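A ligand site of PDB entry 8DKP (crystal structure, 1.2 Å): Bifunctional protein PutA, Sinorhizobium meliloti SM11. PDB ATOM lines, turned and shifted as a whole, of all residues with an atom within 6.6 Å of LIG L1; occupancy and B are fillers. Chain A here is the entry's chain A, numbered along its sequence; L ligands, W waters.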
ATOM      1  N   ASP A  95     -30.450  12.607  23.011  1.00  0.00           N
ATOM      2  CA  ASP A  95     -30.855  11.353  23.630  1.00  0.00           C
ATOM      3  C   ASP A  95     -31.982  11.618  24.612  1.00  0.00           C
ATOM      4  O   ASP A  95     -31.770  12.267  25.635  1.00  0.00           O
ATOM      5  CB  ASP A  95     -29.684  10.723  24.370  1.00  0.00           C
ATOM      6  CG  ASP A  95     -30.116   9.545  25.216  1.00  0.00           C
ATOM      7  OD1 ASP A  95     -30.682   8.592  24.640  1.00  0.00           O
ATOM      8  OD2 ASP A  95     -29.908   9.585  26.446  1.00  0.00           O
ATOM      9  N   GLU A  99     -33.559   3.821  29.738  1.00  0.00           N
ATOM     10  CA  GLU A  99     -32.843   2.594  29.419  1.00  0.00           C
ATOM     11  C   GLU A  99     -33.411   1.485  30.284  1.00  0.00           C
ATOM     12  O   GLU A  99     -34.121   1.732  31.258  1.00  0.00           O
ATOM     13  CB  GLU A  99     -31.336   2.747  29.672  1.00  0.00           C
ATOM     14  CG  GLU A  99     -30.989   3.035  31.122  1.00  0.00           C
ATOM     15  CD  GLU A  99     -29.553   3.498  31.295  1.00  0.00           C
ATOM     16  OE1 GLU A  99     -29.152   4.478  30.641  1.00  0.00           O
ATOM     17  OE2 GLU A  99     -28.830   2.869  32.099  1.00  0.00           O
ATOM     18  N   SER A 137     -29.952   9.693  19.219  1.00  0.00           N
ATOM     19  CA  SER A 137     -29.369   8.445  19.718  1.00  0.00           C
ATOM     20  C   SER A 137     -30.431   7.698  20.507  1.00  0.00           C
ATOM     21  O   SER A 137     -31.228   8.313  21.219  1.00  0.00           O
ATOM     22  CB  SER A 137     -28.178   8.743  20.637  1.00  0.00           C
ATOM     23  OG  SER A 137     -27.051   9.167  19.888  1.00  0.00           O
ATOM     24  N   LYS A 139     -31.271   3.834  22.813  1.00  0.00           N
ATOM     25  CA  LYS A 139     -30.793   2.638  23.498  1.00  0.00           C
ATOM     26  C   LYS A 139     -31.794   1.522  23.266  1.00  0.00           C
ATOM     27  O   LYS A 139     -32.973   1.677  23.600  1.00  0.00           O
ATOM     28  CB  LYS A 139     -30.599   2.894  24.988  1.00  0.00           C
ATOM     29  CG  LYS A 139     -29.295   3.622  25.301  1.00  0.00           C
ATOM     30  CD  LYS A 139     -29.182   3.961  26.782  1.00  0.00           C
ATOM     31  CE  LYS A 139     -27.767   4.384  27.168  1.00  0.00           C
ATOM     32  NZ  LYS A 139     -27.331   5.680  26.575  1.00  0.00           N
ATOM     33  N   ASN A 178     -28.650   6.961  15.756  1.00  0.00           N
ATOM     34  CA  ASN A 178     -27.552   6.170  16.282  1.00  0.00           C
ATOM     35  C   ASN A 178     -28.037   5.178  17.336  1.00  0.00           C
ATOM     36  O   ASN A 178     -28.790   5.561  18.241  1.00  0.00           O
ATOM     37  CB  ASN A 178     -26.501   7.066  16.928  1.00  0.00           C
ATOM     38  CG  ASN A 178     -25.418   6.276  17.607  1.00  0.00           C
ATOM     39  OD1 ASN A 178     -24.497   5.783  16.965  1.00  0.00           O
ATOM     40  ND2 ASN A 178     -25.533   6.117  18.921  1.00  0.00           N
ATOM     41  N   ASP A 180     -26.899   3.410  20.487  1.00  0.00           N
ATOM     42  CA  ASP A 180     -25.874   3.402  21.526  1.00  0.00           C
ATOM     43  C   ASP A 180     -25.467   1.961  21.852  1.00  0.00           C
ATOM     44  O   ASP A 180     -26.276   1.030  21.764  1.00  0.00           O
ATOM     45  CB  ASP A 180     -26.435   4.040  22.791  1.00  0.00           C
ATOM     46  CG  ASP A 180     -26.568   5.559  22.732  1.00  0.00           C
ATOM     47  OD1 ASP A 180     -26.099   6.185  21.759  1.00  0.00           O
ATOM     48  OD2 ASP A 180     -27.165   6.108  23.685  1.00  0.00           O
ATOM     49  N   ALA A 181     -24.216   1.799  22.286  1.00  0.00           N
ATOM     50  CA  ALA A 181     -23.711   0.486  22.712  1.00  0.00           C
ATOM     51  C   ALA A 181     -23.877   0.343  24.216  1.00  0.00           C
ATOM     52  O   ALA A 181     -23.531   1.258  24.979  1.00  0.00           O
ATOM     53  CB  ALA A 181     -22.246   0.334  22.329  1.00  0.00           C
ATOM     54  N   VAL A 212     -22.531   2.409  17.551  1.00  0.00           N
ATOM     55  CA  VAL A 212     -21.378   2.624  18.436  1.00  0.00           C
ATOM     56  C   VAL A 212     -20.591   1.330  18.559  1.00  0.00           C
ATOM     57  O   VAL A 212     -21.178   0.250  18.678  1.00  0.00           O
ATOM     58  CB  VAL A 212     -21.860   3.065  19.824  1.00  0.00           C
ATOM     59  CG1 VAL A 212     -20.680   3.224  20.778  1.00  0.00           C
ATOM     60  CG2 VAL A 212     -22.678   4.338  19.743  1.00  0.00           C
ATOM     61  N   ARG A 241     -19.673   5.406  15.568  1.00  0.00           N
ATOM     62  CA  ARG A 241     -19.161   6.133  16.724  1.00  0.00           C
ATOM     63  C   ARG A 241     -18.178   5.231  17.471  1.00  0.00           C
ATOM     64  O   ARG A 241     -18.570   4.221  18.050  1.00  0.00           O
ATOM     65  CB  ARG A 241     -20.287   6.583  17.629  1.00  0.00           C
ATOM     66  CG  ARG A 241     -19.766   7.427  18.775  1.00  0.00           C
ATOM     67  CD  ARG A 241     -20.743   7.510  19.942  1.00  0.00           C
ATOM     68  NE  ARG A 241     -21.916   8.284  19.560  1.00  0.00           N
ATOM     69  CZ  ARG A 241     -23.114   8.179  20.121  1.00  0.00           C
ATOM     70  NH1 ARG A 241     -23.345   7.336  21.126  1.00  0.00           N
ATOM     71  NH2 ARG A 241     -24.116   8.920  19.651  1.00  0.00           N
ATOM     72  N   ALA A 246     -18.593   2.883  28.447  1.00  0.00           N
ATOM     73  CA  ALA A 246     -19.163   3.490  29.641  1.00  0.00           C
ATOM     74  C   ALA A 246     -19.494   2.524  30.777  1.00  0.00           C
ATOM     75  O   ALA A 246     -19.881   2.987  31.836  1.00  0.00           O
ATOM     76  CB  ALA A 246     -20.444   4.264  29.283  1.00  0.00           C
ATOM     77  N   TYR A 247     -19.340   1.211  30.583  1.00  0.00           N
ATOM     78  CA  TYR A 247     -19.846   0.197  31.505  1.00  0.00           C
ATOM     79  C   TYR A 247     -18.733  -0.666  32.083  1.00  0.00           C
ATOM     80  O   TYR A 247     -18.977  -1.791  32.515  1.00  0.00           O
ATOM     81  CB  TYR A 247     -20.913  -0.678  30.839  1.00  0.00           C
ATOM     82  CG  TYR A 247     -22.055   0.110  30.229  1.00  0.00           C
ATOM     83  CD1 TYR A 247     -21.944   0.668  28.969  1.00  0.00           C
ATOM     84  CD2 TYR A 247     -23.247   0.301  30.915  1.00  0.00           C
ATOM     85  CE1 TYR A 247     -22.975   1.416  28.395  1.00  0.00           C
ATOM     86  CE2 TYR A 247     -24.295   1.025  30.344  1.00  0.00           C
ATOM     87  CZ  TYR A 247     -24.152   1.585  29.101  1.00  0.00           C
ATOM     88  OH  TYR A 247     -25.194   2.323  28.570  1.00  0.00           O
ATOM     89  N   LEU A 323     -19.617  14.512  25.135  1.00  0.00           N
ATOM     90  CA  LEU A 323     -20.824  14.556  25.955  1.00  0.00           C
ATOM     91  C   LEU A 323     -21.092  15.987  26.427  1.00  0.00           C
ATOM     92  O   LEU A 323     -20.166  16.695  26.846  1.00  0.00           O
ATOM     93  CB  LEU A 323     -20.715  13.636  27.179  1.00  0.00           C
ATOM     94  CG  LEU A 323     -20.482  12.142  26.945  1.00  0.00           C
ATOM     95  CD1 LEU A 323     -20.353  11.375  28.242  1.00  0.00           C
ATOM     96  CD2 LEU A 323     -21.555  11.516  26.075  1.00  0.00           C
ATOM     97  N   TYR A 347     -23.380  14.942  22.324  1.00  0.00           N
ATOM     98  CA  TYR A 347     -24.410  14.013  22.786  1.00  0.00           C
ATOM     99  C   TYR A 347     -25.172  14.748  23.881  1.00  0.00           C
ATOM    100  O   TYR A 347     -24.578  15.116  24.907  1.00  0.00           O
ATOM    101  CB  TYR A 347     -23.737  12.746  23.324  1.00  0.00           C
ATOM    102  CG  TYR A 347     -24.686  11.623  23.682  1.00  0.00           C
ATOM    103  CD1 TYR A 347     -25.364  11.619  24.888  1.00  0.00           C
ATOM    104  CD2 TYR A 347     -24.907  10.563  22.808  1.00  0.00           C
ATOM    105  CE1 TYR A 347     -26.247  10.601  25.217  1.00  0.00           C
ATOM    106  CE2 TYR A 347     -25.778   9.533  23.139  1.00  0.00           C
ATOM    107  CZ  TYR A 347     -26.438   9.562  24.346  1.00  0.00           C
ATOM    108  OH  TYR A 347     -27.327   8.561  24.707  1.00  0.00           O
ATOM    109  N   ALA A 358     -29.458   6.923  36.072  1.00  0.00           N
ATOM    110  CA  ALA A 358     -28.511   5.878  35.658  1.00  0.00           C
ATOM    111  C   ALA A 358     -27.381   6.447  34.821  1.00  0.00           C
ATOM    112  O   ALA A 358     -26.210   6.075  34.984  1.00  0.00           O
ATOM    113  CB  ALA A 358     -29.238   4.774  34.894  1.00  0.00           C
ATOM    114  N   TYR A 359     -27.721   7.348  33.901  1.00  0.00           N
ATOM    115  CA  TYR A 359     -26.707   8.023  33.097  1.00  0.00           C
ATOM    116  C   TYR A 359     -25.744   8.792  33.995  1.00  0.00           C
ATOM    117  O   TYR A 359     -24.536   8.777  33.782  1.00  0.00           O
ATOM    118  CB  TYR A 359     -27.431   8.937  32.084  1.00  0.00           C
ATOM    119  CG  TYR A 359     -26.561   9.750  31.164  1.00  0.00           C
ATOM    120  CD1 TYR A 359     -26.119  11.018  31.537  1.00  0.00           C
ATOM    121  CD2 TYR A 359     -26.233   9.298  29.884  1.00  0.00           C
ATOM    122  CE1 TYR A 359     -25.340  11.781  30.715  1.00  0.00           C
ATOM    123  CE2 TYR A 359     -25.466  10.056  29.050  1.00  0.00           C
ATOM    124  CZ  TYR A 359     -25.026  11.297  29.455  1.00  0.00           C
ATOM    125  OH  TYR A 359     -24.263  12.036  28.590  1.00  0.00           O
ATOM    126  N   ARG A 362     -22.948   6.548  35.473  1.00  0.00           N
ATOM    127  CA  ARG A 362     -21.830   6.317  34.578  1.00  0.00           C
ATOM    128  C   ARG A 362     -20.946   7.557  34.430  1.00  0.00           C
ATOM    129  O   ARG A 362     -19.725   7.426  34.293  1.00  0.00           O
ATOM    130  CB  ARG A 362     -22.323   5.800  33.226  1.00  0.00           C
ATOM    131  CG  ARG A 362     -22.987   4.440  33.346  1.00  0.00           C
ATOM    132  CD  ARG A 362     -23.330   3.842  32.001  1.00  0.00           C
ATOM    133  NE  ARG A 362     -24.319   4.640  31.283  1.00  0.00           N
ATOM    134  CZ  ARG A 362     -25.638   4.511  31.424  1.00  0.00           C
ATOM    135  NH1 ARG A 362     -26.160   3.622  32.253  1.00  0.00           N
ATOM    136  NH2 ARG A 362     -26.440   5.285  30.711  1.00  0.00           N
ATOM    137  N   ARG A 363     -21.524   8.754  34.521  1.00  0.00           N
ATOM    138  CA  ARG A 363     -20.688   9.949  34.486  1.00  0.00           C
ATOM    139  C   ARG A 363     -19.830  10.058  35.735  1.00  0.00           C
ATOM    140  O   ARG A 363     -18.705  10.556  35.662  1.00  0.00           O
ATOM    141  CB  ARG A 363     -21.528  11.199  34.271  1.00  0.00           C
ATOM    142  CG  ARG A 363     -22.409  11.200  33.003  1.00  0.00           C
ATOM    143  CD  ARG A 363     -21.644  11.348  31.668  1.00  0.00           C
ATOM    144  NE  ARG A 363     -20.962  10.122  31.278  1.00  0.00           N
ATOM    145  CZ  ARG A 363     -21.577   9.042  30.821  1.00  0.00           C
ATOM    146  NH1 ARG A 363     -22.895   8.961  30.758  1.00  0.00           N
ATOM    147  NH2 ARG A 363     -20.837   8.015  30.393  1.00  0.00           N
ATOM    148  N   GLU A 366     -16.983   7.753  35.358  1.00  0.00           N
ATOM    149  CA  GLU A 366     -16.096   8.290  34.340  1.00  0.00           C
ATOM    150  C   GLU A 366     -15.269   9.459  34.888  1.00  0.00           C
ATOM    151  O   GLU A 366     -14.032   9.478  34.743  1.00  0.00           O
ATOM    152  CB  GLU A 366     -16.923   8.748  33.143  1.00  0.00           C
ATOM    153  CG  GLU A 366     -16.111   9.360  32.020  1.00  0.00           C
ATOM    154  CD  GLU A 366     -16.981   9.707  30.821  1.00  0.00           C
ATOM    155  OE1 GLU A 366     -18.225   9.496  30.882  1.00  0.00           O
ATOM    156  OE2 GLU A 366     -16.421  10.161  29.810  1.00  0.00           O
HETATM  157  O1  LIG L   1     -23.789   5.956  25.991  1.00  0.00           O
HETATM  158  C1  LIG L   1     -23.036   6.421  27.112  1.00  0.00           C
HETATM  159  C2  LIG L   1     -23.896   6.410  28.376  1.00  0.00           C
HETATM  160  O2  LIG L   1     -25.140   6.285  28.310  1.00  0.00           O
HETATM  161  C3  LIG L   1     -22.580   7.819  26.805  1.00  0.00           C
HETATM  162  C4  LIG L   1     -23.605   8.343  25.855  1.00  0.00           C
HETATM  163  C5  LIG L   1     -24.181   7.098  25.192  1.00  0.00           C
HETATM  164  O3  LIG L   1     -23.330   6.545  29.485  1.00  0.00           O
HETATM  165  P1  LG2 L   2     -10.215   8.471  28.843  1.00  0.00           P
HETATM  166  O1  LG2 L   2      -9.926   8.992  30.253  1.00  0.00           O
HETATM  167  O2  LG2 L   2      -9.100   8.496  27.884  1.00  0.00           O
HETATM  168  O3  LG2 L   2     -10.629   7.029  28.902  1.00  0.00           O
HETATM  169  C1  LG2 L   2     -11.493   6.530  29.955  1.00  0.00           C
HETATM  170  C2  LG2 L   2     -12.048   5.153  29.575  1.00  0.00           C
HETATM  171  O4  LG2 L   2     -11.074   4.136  29.684  1.00  0.00           O
HETATM  172  C3  LG2 L   2     -13.184   4.678  30.426  1.00  0.00           C
HETATM  173  O5  LG2 L   2     -14.397   5.314  30.097  1.00  0.00           O
HETATM  174  C4  LG2 L   2     -13.181   3.214  30.109  1.00  0.00           C
HETATM  175  O6  LG2 L   2     -13.757   2.940  28.875  1.00  0.00           O
HETATM  176  C5  LG2 L   2     -11.724   2.928  29.968  1.00  0.00           C
HETATM  177  N1  LG2 L   2     -11.067   2.339  31.114  1.00  0.00           N
HETATM  178  C6  LG2 L   2     -10.878   2.934  32.332  1.00  0.00           C
HETATM  179  N2  LG2 L   2     -10.196   2.091  33.139  1.00  0.00           N
HETATM  180  C7  LG2 L   2      -9.922   0.928  32.424  1.00  0.00           C
HETATM  181  C8  LG2 L   2      -9.251  -0.251  32.699  1.00  0.00           C
HETATM  182  N3  LG2 L   2      -8.661  -0.462  34.005  1.00  0.00           N
HETATM  183  N4  LG2 L   2      -9.132  -1.210  31.779  1.00  0.00           N
HETATM  184  C9  LG2 L   2      -9.676  -1.045  30.542  1.00  0.00           C
HETATM  185  N5  LG2 L   2     -10.336   0.114  30.198  1.00  0.00           N
HETATM  186  C10 LG2 L   2     -10.467   1.075  31.111  1.00  0.00           C
HETATM  187  N6  LG2 L   2     -19.749   4.385  25.759  1.00  0.00           N
HETATM  188  C11 LG2 L   2     -20.596   3.286  25.605  1.00  0.00           C
HETATM  189  O7  LG2 L   2     -20.339   2.187  26.296  1.00  0.00           O
HETATM  190  N7  LG2 L   2     -21.660   3.307  24.763  1.00  0.00           N
HETATM  191  C12 LG2 L   2     -21.952   4.425  24.055  1.00  0.00           C
HETATM  192  O8  LG2 L   2     -22.981   4.417  23.225  1.00  0.00           O
HETATM  193  C13 LG2 L   2     -21.138   5.634  24.192  1.00  0.00           C
HETATM  194  N8  LG2 L   2     -21.410   6.807  23.508  1.00  0.00           N
HETATM  195  C14 LG2 L   2     -20.586   7.886  23.702  1.00  0.00           C
HETATM  196  C15 LG2 L   2     -20.858   9.087  23.032  1.00  0.00           C
HETATM  197  C16 LG2 L   2     -20.029  10.189  23.203  1.00  0.00           C
HETATM  198  C17 LG2 L   2     -20.312  11.483  22.457  1.00  0.00           C
HETATM  199  C18 LG2 L   2     -18.932  10.117  24.035  1.00  0.00           C
HETATM  200  C19 LG2 L   2     -18.012  11.284  24.231  1.00  0.00           C
HETATM  201  C20 LG2 L   2     -18.667   8.929  24.725  1.00  0.00           C
HETATM  202  C21 LG2 L   2     -19.486   7.828  24.552  1.00  0.00           C
HETATM  203  N9  LG2 L   2     -19.201   6.619  25.238  1.00  0.00           N
HETATM  204  C22 LG2 L   2     -20.010   5.528  25.069  1.00  0.00           C
HETATM  205  C23 LG2 L   2     -17.991   6.512  26.052  1.00  0.00           C
HETATM  206  C24 LG2 L   2     -18.088   6.712  27.542  1.00  0.00           C
HETATM  207  O9  LG2 L   2     -19.287   7.310  27.865  1.00  0.00           O
HETATM  208  C25 LG2 L   2     -16.929   7.619  27.988  1.00  0.00           C
HETATM  209  O10 LG2 L   2     -17.256   8.924  27.645  1.00  0.00           O
HETATM  210  C26 LG2 L   2     -15.572   7.253  27.406  1.00  0.00           C
HETATM  211  O11 LG2 L   2     -15.332   5.890  27.511  1.00  0.00           O
HETATM  212  C27 LG2 L   2     -14.453   8.097  28.000  1.00  0.00           C
HETATM  213  O12 LG2 L   2     -13.300   7.981  27.189  1.00  0.00           O
HETATM  214  P2  LG2 L   2     -12.323   9.177  26.907  1.00  0.00           P
HETATM  215  O13 LG2 L   2     -11.434   8.917  25.670  1.00  0.00           O
HETATM  216  O14 LG2 L   2     -13.082  10.506  27.024  1.00  0.00           O
HETATM  217  O15 LG2 L   2     -11.434   9.176  28.220  1.00  0.00           O
HETATM  218  O   HOH W   1     -24.942   3.472  26.072  1.00  0.00           O
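The side-chain carboxylate (OE2) of Glu 99 lies within salt-bridge range of the guanidinium group (NH1) of Arg 362 (2.8 Å). The side-chain carboxylate (OD1) of Asp 180 is in salt-bridge range of the guanidinium group (NH1) of Arg 241, 3.1 Å away. The side-chain carboxylate of Asp 180 is in salt-bridge range of the side-chain amino group of Lys 139, 2.9 Å away. OH of Tyr 347 sits close to OD2 of Asp 95 (3.3 Å). The side-chain amide nitrogen of Asn 178 sits at hydrogen-bond distance from the side-chain carboxylate of Asp 180, 2.9 Å away. The side-chain hydroxyl of Tyr 347 sits at hydrogen-bond distance from the side-chain carboxylate of Asp 180 (2.7 Å). The guanidinium group (NH1) of Arg 363 sits close to the backbone carbonyl oxygen (O) of Tyr 359, 3.4 Å away. NZ of Lys 139 sits at hydrogen-bond distance from OH of Tyr 347, at 3.4 Å.
Water W1 lies within hydrogen-bond range of an oxygen (O1) of LIG L1 (2.7 Å), the side-chain hydroxyl (OH) of Tyr 247 (2.8 Å), the backbone carbonyl oxygen (O) of Ala 181 (2.8 Å) and the side-chain amino group (NZ) of Lys 139 (3.3 Å).
Merely in contact with LIG L1: Tyr 347 (3.4 Å), Asp 180 (3.5 Å), Tyr 359 (3.6 Å), Ala 246 (3.7 Å), Leu 323 (3.8 Å) and Tyr 247 (3.97 Å). Hydrophobic or aromatic side chains within 4 Å of LIG L1: Ala 246, Leu 323, Tyr 347 and Tyr 359. Nine residues have an atom within 4 Å of LIG L1: Lys 139, Asp 180, Ala 246, Tyr 247, Leu 323, Tyr 347, Tyr 359, Arg 362 and Arg 363. The nearest printed residue that does not touch LIG L1 is Arg 241 (4.2 Å).
An oxygen (O7) of LG2 L2 lies within hydrogen-bond range of the backbone NH (N) of Ala 246, 2.9 Å away. OE2 of Glu 366 sits at hydrogen-bond distance from O10 of LG2 L2, at 2.6 Å. The side-chain amino group (NZ) of Lys 139 lies within salt-bridge range of an oxygen (O2) of LIG L1, 2.9 Å away. The backbone NH (N) of Ala 181 lies within hydrogen-bond range of an oxygen (O8) of LG2 L2 (3.0 Å). O3 of LIG L1 lies within salt-bridge range of NE of Arg 362, 2.8 Å away. The guanidinium group (NH1) of Arg 241 lies within hydrogen-bond range of a nitrogen (N8) of LG2 L2, at 3.1 Å. O9 of LG2 L2 sits at hydrogen-bond distance from NH2 of Arg 363 (3.0 Å). An oxygen (O3) of LIG L1 is in salt-bridge range of the guanidinium group (NH1) of Arg 363, 2.8 Å away. A nitrogen (N7) of LG2 L2 sits at hydrogen-bond distance from the backbone carbonyl oxygen of Ala 181, 2.8 Å away.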
